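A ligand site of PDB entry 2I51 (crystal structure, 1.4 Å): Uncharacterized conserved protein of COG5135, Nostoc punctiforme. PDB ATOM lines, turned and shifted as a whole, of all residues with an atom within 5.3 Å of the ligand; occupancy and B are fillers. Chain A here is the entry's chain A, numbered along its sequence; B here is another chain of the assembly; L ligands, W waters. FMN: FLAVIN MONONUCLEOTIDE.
Water W2 lies within hydrogen-bond range of O3' of the ligand (2.7 Å), OD2 of Asp 166 of chain B (2.7 Å), NH1 of Arg 89 of chain B (3.1 Å) and NH2 of Arg 177 of chain B (3.5 Å).
Water W1 lies within hydrogen-bond range of O4 of the ligand (2.7 Å), O of Val 44 (2.7 Å), N of Ile 58 (3.0 Å) and NE of Arg 46 (3.1 Å).
Water W5 lies within hydrogen-bond range of an oxygen (O2) of the ligand (2.7 Å), the side-chain hydroxyl (OG1) of Thr 59 (2.8 Å), the backbone NH (N) of Asp 60 (3.0 Å) and the side-chain amino group (NZ) of Lys 65 (3.3 Å).
Water W4 lies within hydrogen-bond range of OXT of Pro 195 of chain B and O3' of the ligand.
Water W9 bridges OXT of Pro 195 of chain B (2.7 Å) and NH1 of Arg 177 of chain B (3.4 Å).
Water W7 lies within hydrogen-bond range of the side-chain amide nitrogen of Gln 68 (2.9 Å), the guanidinium group of Arg 89 of chain B (3.0 Å) and an oxygen (O3P) of the ligand (3.3 Å).
Tyr 26 touches the ligand (CD2 to C7M, 3.4 Å).
Leu 43 touches the ligand.
CE1 of Tyr 80 of chain B touches C8M of the ligand (3.6 Å).
Leu 168 of chain B touches the ligand.
Leu 170 of chain B touches the ligand (CD1 to C7M, 3.9 Å).
Hydrophobic or aromatic side chains that line the ligand: Tyr 26, Leu 43, Val 44, Ala 64, Tyr 80 of chain B, Leu 168 of chain B and Leu 170 of chain B.
An oxygen (O2') of the ligand lies within hydrogen-bond range of the backbone NH of Thr 42 (3.5 Å).
The backbone NH of Ala 64 sits at hydrogen-bond distance from an oxygen (O1P) of the ligand (3.3 Å).
The side-chain hydroxyl (OG1) of Thr 59 is in hydrogen-bond range of an oxygen (O2) of the ligand.
The side-chain amide nitrogen (NE2) of Gln 87 of chain B lies within hydrogen-bond range of an oxygen (O2') of the ligand (3.0 Å).
N of Lys 65 lies within hydrogen-bond range of O1P of the ligand, at 2.9 Å.
The guanidinium group of Arg 89 of chain B lies within salt-bridge range of an oxygen (O3P) of the ligand (3.1 Å).
The backbone carbonyl oxygen (O) of Thr 42 lies within hydrogen-bond range of an oxygen (O2') of the ligand (2.8 Å).
An oxygen (O3P) of the ligand lies within salt-bridge range of the guanidinium group of Arg 41.
NH2 of Arg 177 of chain B is in salt-bridge range of O2P of the ligand (3.9 Å).
The side-chain hydroxyl of Ser 63 sits close to an oxygen (O1P) of the ligand.
An oxygen (O1P) of the ligand lies within salt-bridge range of the side-chain amino group of Lys 65 (2.8 Å).
The backbone carbonyl oxygen (O) of Ile 58 is in hydrogen-bond range of a nitrogen (N3) of the ligand (2.9 Å).
N of Val 44 is in hydrogen-bond range of O4 of the ligand (3.1 Å).
The side-chain hydroxyl (OG) of Ser 63 lies within hydrogen-bond range of the side-chain amino group (NZ) of Lys 65, at 3.0 Å.
The side-chain carboxylate (OD2) of Asp 166 of chain B is in salt-bridge range of the guanidinium group (NH1) of Arg 89 of chain B (3.99 Å).
OE1 of Gln 87 of chain B sits at hydrogen-bond distance from OG1 of Thr 42.
The side-chain carboxylate of Asp 166 of chain B lies within salt-bridge range of the guanidinium group of Arg 177 of chain B, 2.8 Å away.
The side-chain hydroxyl (OG) of Ser 63 lies within hydrogen-bond range of the backbone carbonyl oxygen (O) of Asp 60 (2.8 Å).
The side-chain amide oxygen of Gln 68 sits at hydrogen-bond distance from the guanidinium group of Arg 41, 2.9 Å away.
N of Gln 87 of chain B sits at hydrogen-bond distance from O of Leu 168 of chain B, 2.8 Å away.
OG1 of Thr 59 is in hydrogen-bond range of NZ of Lys 65, 2.8 Å away.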
ATOM      1  N   TYR A  26     -29.174   8.249  15.447  1.00  0.00           N
ATOM      2  CA  TYR A  26     -28.996   8.043  16.866  1.00  0.00           C
ATOM      3  C   TYR A  26     -30.365   8.011  17.530  1.00  0.00           C
ATOM      4  O   TYR A  26     -31.248   8.839  17.220  1.00  0.00           O
ATOM      5  CB  TYR A  26     -28.179   9.150  17.496  1.00  0.00           C
ATOM      6  CG  TYR A  26     -26.810   9.370  16.952  1.00  0.00           C
ATOM      7  CD1 TYR A  26     -26.176   8.441  16.181  1.00  0.00           C
ATOM      8  CD2 TYR A  26     -26.165  10.561  17.222  1.00  0.00           C
ATOM      9  CE1 TYR A  26     -24.894   8.719  15.647  1.00  0.00           C
ATOM     10  CE2 TYR A  26     -24.927  10.830  16.729  1.00  0.00           C
ATOM     11  CZ  TYR A  26     -24.301   9.921  15.956  1.00  0.00           C
ATOM     12  OH  TYR A  26     -23.026  10.198  15.429  1.00  0.00           O
ATOM     13  N   ARG A  41     -30.451   5.488  27.292  1.00  0.00           N
ATOM     14  CA  ARG A  41     -29.181   5.938  26.672  1.00  0.00           C
ATOM     15  C   ARG A  41     -29.264   5.905  25.182  1.00  0.00           C
ATOM     16  O   ARG A  41     -30.047   5.155  24.607  1.00  0.00           O
ATOM     17  CB  ARG A  41     -27.998   5.110  27.151  1.00  0.00           C
ATOM     18  CG  ARG A  41     -27.831   3.790  26.494  1.00  0.00           C
ATOM     19  CD  ARG A  41     -28.862   2.749  26.884  1.00  0.00           C
ATOM     20  NE  ARG A  41     -28.764   2.285  28.261  1.00  0.00           N
ATOM     21  CZ  ARG A  41     -29.657   1.581  28.951  1.00  0.00           C
ATOM     22  NH1 ARG A  41     -30.920   1.409  28.506  1.00  0.00           N
ATOM     23  NH2 ARG A  41     -29.315   1.105  30.116  1.00  0.00           N
ATOM     24  N   THR A  42     -28.389   6.679  24.545  1.00  0.00           N
ATOM     25  CA  THR A  42     -28.326   6.748  23.115  1.00  0.00           C
ATOM     26  C   THR A  42     -27.549   5.574  22.542  1.00  0.00           C
ATOM     27  O   THR A  42     -26.495   5.195  23.112  1.00  0.00           O
ATOM     28  CB  THR A  42     -27.695   8.083  22.659  1.00  0.00           C
ATOM     29  OG1 THR A  42     -28.457   9.169  23.211  1.00  0.00           O
ATOM     30  CG2 THR A  42     -27.676   8.213  21.131  1.00  0.00           C
ATOM     31  N   LEU A  43     -28.053   5.024  21.432  1.00  0.00           N
ATOM     32  CA  LEU A  43     -27.334   4.059  20.642  1.00  0.00           C
ATOM     33  C   LEU A  43     -27.374   4.478  19.197  1.00  0.00           C
ATOM     34  O   LEU A  43     -28.218   5.255  18.791  1.00  0.00           O
ATOM     35  CB  LEU A  43     -27.996   2.681  20.677  1.00  0.00           C
ATOM     36  CG  LEU A  43     -28.359   2.128  22.047  1.00  0.00           C
ATOM     37  CD1 LEU A  43     -29.192   0.818  21.888  1.00  0.00           C
ATOM     38  CD2 LEU A  43     -27.101   1.945  22.769  1.00  0.00           C
ATOM     39  N   VAL A  44     -26.474   3.954  18.364  1.00  0.00           N
ATOM     40  CA  VAL A  44     -26.540   4.109  16.904  1.00  0.00           C
ATOM     41  C   VAL A  44     -27.365   3.013  16.271  1.00  0.00           C
ATOM     42  O   VAL A  44     -27.104   1.823  16.502  1.00  0.00           O
ATOM     43  CB  VAL A  44     -25.106   4.014  16.314  1.00  0.00           C
ATOM     44  CG1 VAL A  44     -25.133   4.148  14.764  1.00  0.00           C
ATOM     45  CG2 VAL A  44     -24.189   5.093  16.939  1.00  0.00           C
ATOM     46  N   ARG A  46     -28.141   0.591  13.456  1.00  0.00           N
ATOM     47  CA  ARG A  46     -27.273  -0.078  12.488  1.00  0.00           C
ATOM     48  C   ARG A  46     -28.048  -0.884  11.457  1.00  0.00           C
ATOM     49  O   ARG A  46     -27.593  -1.949  11.017  1.00  0.00           O
ATOM     50  CB  ARG A  46     -26.282  -0.955  13.232  1.00  0.00           C
ATOM     51  CG  ARG A  46     -25.559  -0.187  14.343  1.00  0.00           C
ATOM     52  CD  ARG A  46     -24.165  -0.577  14.557  1.00  0.00           C
ATOM     53  NE  ARG A  46     -23.392   0.383  15.352  1.00  0.00           N
ATOM     54  CZ  ARG A  46     -22.335   1.074  14.877  1.00  0.00           C
ATOM     55  NH1 ARG A  46     -21.980   0.980  13.612  1.00  0.00           N
ATOM     56  NH2 ARG A  46     -21.665   1.903  15.651  1.00  0.00           N
ATOM     57  N   ILE A  58     -25.264  -2.521  18.428  1.00  0.00           N
ATOM     58  CA  ILE A  58     -24.171  -3.215  19.086  1.00  0.00           C
ATOM     59  C   ILE A  58     -23.994  -2.659  20.483  1.00  0.00           C
ATOM     60  O   ILE A  58     -24.341  -1.485  20.749  1.00  0.00           O
ATOM     61  CB  ILE A  58     -22.860  -3.103  18.280  1.00  0.00           C
ATOM     62  CG1 ILE A  58     -22.255  -1.708  18.307  1.00  0.00           C
ATOM     63  CG2 ILE A  58     -23.072  -3.658  16.880  1.00  0.00           C
ATOM     64  CD1 ILE A  58     -20.933  -1.514  17.501  1.00  0.00           C
ATOM     65  N   THR A  59     -23.459  -3.490  21.358  1.00  0.00           N
ATOM     66  CA  THR A  59     -23.146  -3.058  22.718  1.00  0.00           C
ATOM     67  C   THR A  59     -22.103  -3.981  23.298  1.00  0.00           C
ATOM     68  O   THR A  59     -21.831  -5.060  22.765  1.00  0.00           O
ATOM     69  CB  THR A  59     -24.388  -2.928  23.595  1.00  0.00           C
ATOM     70  OG1 THR A  59     -24.129  -2.042  24.693  1.00  0.00           O
ATOM     71  CG2 THR A  59     -24.885  -4.288  24.085  1.00  0.00           C
ATOM     72  N   ASP A  60     -21.497  -3.537  24.387  1.00  0.00           N
ATOM     73  CA  ASP A  60     -20.459  -4.293  25.091  1.00  0.00           C
ATOM     74  C   ASP A  60     -21.092  -5.151  26.194  1.00  0.00           C
ATOM     75  O   ASP A  60     -21.944  -4.662  26.954  1.00  0.00           O
ATOM     76  CB  ASP A  60     -19.466  -3.284  25.669  1.00  0.00           C
ATOM     77  CG  ASP A  60     -18.164  -3.885  26.099  1.00  0.00           C
ATOM     78  OD1 ASP A  60     -18.128  -4.856  26.874  1.00  0.00           O
ATOM     79  OD2 ASP A  60     -17.136  -3.356  25.616  1.00  0.00           O
ATOM     80  N   SER A  63     -21.138  -3.653  29.679  1.00  0.00           N
ATOM     81  CA  SER A  63     -21.973  -2.492  30.024  1.00  0.00           C
ATOM     82  C   SER A  63     -23.167  -2.878  30.924  1.00  0.00           C
ATOM     83  O   SER A  63     -23.637  -4.023  30.982  1.00  0.00           O
ATOM     84  CB  SER A  63     -22.442  -1.788  28.785  1.00  0.00           C
ATOM     85  OG  SER A  63     -23.373  -2.578  28.099  1.00  0.00           O
ATOM     86  N   ALA A  64     -23.656  -1.891  31.680  1.00  0.00           N
ATOM     87  CA  ALA A  64     -24.774  -2.127  32.558  1.00  0.00           C
ATOM     88  C   ALA A  64     -26.013  -2.642  31.848  1.00  0.00           C
ATOM     89  O   ALA A  64     -26.760  -3.461  32.421  1.00  0.00           O
ATOM     90  CB  ALA A  64     -25.128  -0.840  33.307  1.00  0.00           C
ATOM     91  N   LYS A  65     -26.256  -2.154  30.635  1.00  0.00           N
ATOM     92  CA  LYS A  65     -27.491  -2.490  29.955  1.00  0.00           C
ATOM     93  C   LYS A  65     -27.498  -3.983  29.665  1.00  0.00           C
ATOM     94  O   LYS A  65     -28.551  -4.569  29.549  1.00  0.00           O
ATOM     95  CB  LYS A  65     -27.677  -1.720  28.670  1.00  0.00           C
ATOM     96  CG  LYS A  65     -26.856  -2.213  27.447  1.00  0.00           C
ATOM     97  CD  LYS A  65     -26.995  -1.305  26.242  1.00  0.00           C
ATOM     98  CE  LYS A  65     -26.188  -0.045  26.344  1.00  0.00           C
ATOM     99  NZ  LYS A  65     -24.740  -0.215  26.779  1.00  0.00           N
ATOM    100  N   ALA A  66     -26.321  -4.594  29.505  1.00  0.00           N
ATOM    101  CA  ALA A  66     -26.298  -6.048  29.182  1.00  0.00           C
ATOM    102  C   ALA A  66     -27.018  -6.858  30.242  1.00  0.00           C
ATOM    103  O   ALA A  66     -27.873  -7.673  29.919  1.00  0.00           O
ATOM    104  CB  ALA A  66     -24.850  -6.556  28.948  1.00  0.00           C
ATOM    105  N   GLN A  68     -29.132  -5.679  32.465  1.00  0.00           N
ATOM    106  CA  GLN A  68     -30.531  -5.231  32.556  1.00  0.00           C
ATOM    107  C   GLN A  68     -31.359  -5.996  31.518  1.00  0.00           C
ATOM    108  O   GLN A  68     -32.466  -6.434  31.805  1.00  0.00           O
ATOM    109  CB  GLN A  68     -30.675  -3.736  32.292  1.00  0.00           C
ATOM    110  CG  GLN A  68     -29.939  -2.819  33.330  1.00  0.00           C
ATOM    111  CD  GLN A  68     -29.804  -1.392  32.882  1.00  0.00           C
ATOM    112  OE1 GLN A  68     -30.393  -0.966  31.886  1.00  0.00           O
ATOM    113  NE2 GLN A  68     -28.993  -0.626  33.623  1.00  0.00           N
ATOM    114  N   TYR B  80     -29.156  14.338  24.334  1.00  0.00           N
ATOM    115  CA  TYR B  80     -28.042  14.350  23.402  1.00  0.00           C
ATOM    116  C   TYR B  80     -27.962  15.704  22.713  1.00  0.00           C
ATOM    117  O   TYR B  80     -28.952  16.199  22.181  1.00  0.00           O
ATOM    118  CB  TYR B  80     -28.168  13.228  22.368  1.00  0.00           C
ATOM    119  CG  TYR B  80     -26.987  13.200  21.440  1.00  0.00           C
ATOM    120  CD1 TYR B  80     -25.727  12.931  21.939  1.00  0.00           C
ATOM    121  CD2 TYR B  80     -27.110  13.522  20.103  1.00  0.00           C
ATOM    122  CE1 TYR B  80     -24.628  12.961  21.115  1.00  0.00           C
ATOM    123  CE2 TYR B  80     -26.001  13.568  19.252  1.00  0.00           C
ATOM    124  CZ  TYR B  80     -24.758  13.275  19.770  1.00  0.00           C
ATOM    125  OH  TYR B  80     -23.602  13.324  18.957  1.00  0.00           O
ATOM    126  N   GLU B  86     -22.267  15.386  22.887  1.00  0.00           N
ATOM    127  CA  GLU B  86     -22.276  15.007  24.289  1.00  0.00           C
ATOM    128  C   GLU B  86     -23.654  14.617  24.762  1.00  0.00           C
ATOM    129  O   GLU B  86     -24.681  15.055  24.252  1.00  0.00           O
ATOM    130  CB  GLU B  86     -21.750  16.090  25.202  1.00  0.00           C
ATOM    131  CG  GLU B  86     -22.556  17.316  25.235  1.00  0.00           C
ATOM    132  CD  GLU B  86     -21.802  18.508  25.848  1.00  0.00           C
ATOM    133  OE1 GLU B  86     -21.389  18.369  27.016  1.00  0.00           O
ATOM    134  OE2 GLU B  86     -21.668  19.584  25.217  1.00  0.00           O
ATOM    135  N   GLN B  87     -23.653  13.706  25.730  1.00  0.00           N
ATOM    136  CA  GLN B  87     -24.862  13.129  26.279  1.00  0.00           C
ATOM    137  C   GLN B  87     -24.912  13.338  27.795  1.00  0.00           C
ATOM    138  O   GLN B  87     -23.874  13.170  28.477  1.00  0.00           O
ATOM    139  CB  GLN B  87     -24.883  11.616  26.037  1.00  0.00           C
ATOM    140  CG  GLN B  87     -26.025  10.889  26.670  1.00  0.00           C
ATOM    141  CD  GLN B  87     -26.065   9.385  26.287  1.00  0.00           C
ATOM    142  OE1 GLN B  87     -26.802   8.996  25.366  1.00  0.00           O
ATOM    143  NE2 GLN B  87     -25.246   8.616  26.894  1.00  0.00           N
ATOM    144  N   ARG B  89     -27.252  11.834  30.938  1.00  0.00           N
ATOM    145  CA  ARG B  89     -28.285  10.994  31.488  1.00  0.00           C
ATOM    146  C   ARG B  89     -28.519  11.461  32.880  1.00  0.00           C
ATOM    147  O   ARG B  89     -27.540  11.677  33.628  1.00  0.00           O
ATOM    148  CB  ARG B  89     -27.881   9.534  31.461  1.00  0.00           C
ATOM    149  CG  ARG B  89     -27.736   8.963  30.067  1.00  0.00           C
ATOM    150  CD  ARG B  89     -27.010   7.612  30.084  1.00  0.00           C
ATOM    151  NE  ARG B  89     -27.803   6.602  30.784  1.00  0.00           N
ATOM    152  CZ  ARG B  89     -27.432   5.335  30.955  1.00  0.00           C
ATOM    153  NH1 ARG B  89     -26.285   4.945  30.474  1.00  0.00           N
ATOM    154  NH2 ARG B  89     -28.230   4.488  31.558  1.00  0.00           N
ATOM    155  N   ASP B 166     -24.804  11.204  34.485  1.00  0.00           N
ATOM    156  CA  ASP B 166     -23.738  10.565  33.730  1.00  0.00           C
ATOM    157  C   ASP B 166     -23.550  11.423  32.498  1.00  0.00           C
ATOM    158  O   ASP B 166     -24.452  11.511  31.672  1.00  0.00           O
ATOM    159  CB  ASP B 166     -24.196   9.145  33.400  1.00  0.00           C
ATOM    160  CG  ASP B 166     -23.195   8.304  32.626  1.00  0.00           C
ATOM    161  OD1 ASP B 166     -22.141   8.777  32.215  1.00  0.00           O
ATOM    162  OD2 ASP B 166     -23.555   7.116  32.412  1.00  0.00           O
ATOM    163  N   LEU B 168     -21.304  12.125  29.178  1.00  0.00           N
ATOM    164  CA  LEU B 168     -20.403  11.537  28.216  1.00  0.00           C
ATOM    165  C   LEU B 168     -20.082  12.531  27.119  1.00  0.00           C
ATOM    166  O   LEU B 168     -20.998  13.028  26.490  1.00  0.00           O
ATOM    167  CB  LEU B 168     -21.046  10.294  27.614  1.00  0.00           C
ATOM    168  CG  LEU B 168     -20.280   9.591  26.507  1.00  0.00           C
ATOM    169  CD1 LEU B 168     -18.932   8.985  27.011  1.00  0.00           C
ATOM    170  CD2 LEU B 168     -21.108   8.500  25.846  1.00  0.00           C
ATOM    171  N   LEU B 170     -18.213  12.789  23.598  1.00  0.00           N
ATOM    172  CA  LEU B 170     -17.570  12.009  22.558  1.00  0.00           C
ATOM    173  C   LEU B 170     -16.356  12.676  21.969  1.00  0.00           C
ATOM    174  O   LEU B 170     -15.530  11.998  21.326  1.00  0.00           O
ATOM    175  CB  LEU B 170     -18.558  11.699  21.433  1.00  0.00           C
ATOM    176  CG  LEU B 170     -19.811  10.924  21.852  1.00  0.00           C
ATOM    177  CD1 LEU B 170     -20.734  10.646  20.631  1.00  0.00           C
ATOM    178  CD2 LEU B 170     -19.448   9.608  22.496  1.00  0.00           C
ATOM    179  N   ARG B 177     -15.965  10.727  30.364  1.00  0.00           N
ATOM    180  CA  ARG B 177     -17.197  10.369  31.035  1.00  0.00           C
ATOM    181  C   ARG B 177     -17.091  10.651  32.509  1.00  0.00           C
ATOM    182  O   ARG B 177     -16.134  10.265  33.156  1.00  0.00           O
ATOM    183  CB  ARG B 177     -17.520   8.920  30.805  1.00  0.00           C
ATOM    184  CG  ARG B 177     -18.903   8.503  31.164  1.00  0.00           C
ATOM    185  CD  ARG B 177     -19.075   7.037  30.879  1.00  0.00           C
ATOM    186  NE  ARG B 177     -20.376   6.548  31.299  1.00  0.00           N
ATOM    187  CZ  ARG B 177     -20.679   5.264  31.444  1.00  0.00           C
ATOM    188  NH1 ARG B 177     -19.763   4.339  31.203  1.00  0.00           N
ATOM    189  NH2 ARG B 177     -21.882   4.924  31.845  1.00  0.00           N
ATOM    190  N   PRO B 195     -15.259   5.422  29.642  1.00  0.00           N
ATOM    191  CA  PRO B 195     -16.410   5.459  28.700  1.00  0.00           C
ATOM    192  C   PRO B 195     -17.090   4.121  28.498  1.00  0.00           C
ATOM    193  O   PRO B 195     -16.395   3.123  28.339  1.00  0.00           O
ATOM    194  CB  PRO B 195     -15.799   5.969  27.410  1.00  0.00           C
ATOM    195  CG  PRO B 195     -14.532   6.629  27.775  1.00  0.00           C
ATOM    196  CD  PRO B 195     -14.075   6.110  29.097  1.00  0.00           C
ATOM    197  OXT PRO B 195     -18.340   4.007  28.502  1.00  0.00           O
HETATM  198  N1  FMN L   1     -23.438   2.578  23.503  1.00  0.00           N
HETATM  199  C2  FMN L   1     -23.606   1.344  22.991  1.00  0.00           C
HETATM  200  O2  FMN L   1     -23.583   0.333  23.709  1.00  0.00           O
HETATM  201  N3  FMN L   1     -23.866   1.186  21.644  1.00  0.00           N
HETATM  202  C4  FMN L   1     -23.930   2.246  20.789  1.00  0.00           C
HETATM  203  O4  FMN L   1     -24.317   2.100  19.566  1.00  0.00           O
HETATM  204  C4A FMN L   1     -23.758   3.523  21.289  1.00  0.00           C
HETATM  205  N5  FMN L   1     -23.786   4.629  20.460  1.00  0.00           N
HETATM  206  C5A FMN L   1     -23.813   5.908  21.075  1.00  0.00           C
HETATM  207  C6  FMN L   1     -23.959   7.027  20.273  1.00  0.00           C
HETATM  208  C7  FMN L   1     -23.962   8.324  20.808  1.00  0.00           C
HETATM  209  C7M FMN L   1     -24.382   9.492  19.945  1.00  0.00           C
HETATM  210  C8  FMN L   1     -23.749   8.447  22.175  1.00  0.00           C
HETATM  211  C8M FMN L   1     -23.994   9.814  22.846  1.00  0.00           C
HETATM  212  C9  FMN L   1     -23.573   7.327  22.988  1.00  0.00           C
HETATM  213  C9A FMN L   1     -23.560   6.055  22.427  1.00  0.00           C
HETATM  214  N10 FMN L   1     -23.367   4.924  23.199  1.00  0.00           N
HETATM  215  C10 FMN L   1     -23.515   3.683  22.674  1.00  0.00           C
HETATM  216  C1' FMN L   1     -22.949   5.040  24.660  1.00  0.00           C
HETATM  217  C2' FMN L   1     -24.208   4.857  25.517  1.00  0.00           C
HETATM  218  O2' FMN L   1     -25.091   5.998  25.368  1.00  0.00           O
HETATM  219  C3' FMN L   1     -23.904   4.587  27.008  1.00  0.00           C
HETATM  220  O3' FMN L   1     -23.048   5.608  27.468  1.00  0.00           O
HETATM  221  C4' FMN L   1     -23.182   3.220  27.095  1.00  0.00           C
HETATM  222  O4' FMN L   1     -23.712   2.208  26.234  1.00  0.00           O
HETATM  223  C5' FMN L   1     -23.332   2.720  28.527  1.00  0.00           C
HETATM  224  O5' FMN L   1     -24.723   2.574  28.813  1.00  0.00           O
HETATM  225  P   FMN L   1     -25.199   1.582  29.932  1.00  0.00           P
HETATM  226  O1P FMN L   1     -24.982   0.169  29.525  1.00  0.00           O
HETATM  227  O2P FMN L   1     -24.337   1.921  31.196  1.00  0.00           O
HETATM  228  O3P FMN L   1     -26.614   1.918  30.256  1.00  0.00           O
HETATM  229  O   HOH W   1     -25.256   0.359  17.770  1.00  0.00           O
HETATM  230  O   HOH W   2     -23.893   6.761  29.723  1.00  0.00           O
HETATM  231  O   HOH W   3     -20.950   4.357  18.451  1.00  0.00           O
HETATM  232  O   HOH W   4     -20.268   5.348  27.183  1.00  0.00           O
HETATM  233  O   HOH W   5     -21.766  -0.697  25.385  1.00  0.00           O
HETATM  234  O   HOH W   6     -21.931   2.061  18.353  1.00  0.00           O
HETATM  235  O   HOH W   7     -27.986   2.053  33.223  1.00  0.00           O
HETATM  236  O   HOH W   8     -25.405   2.848  33.536  1.00  0.00           O
HETATM  237  O   HOH W   9     -20.229   2.142  28.655  1.00  0.00           O
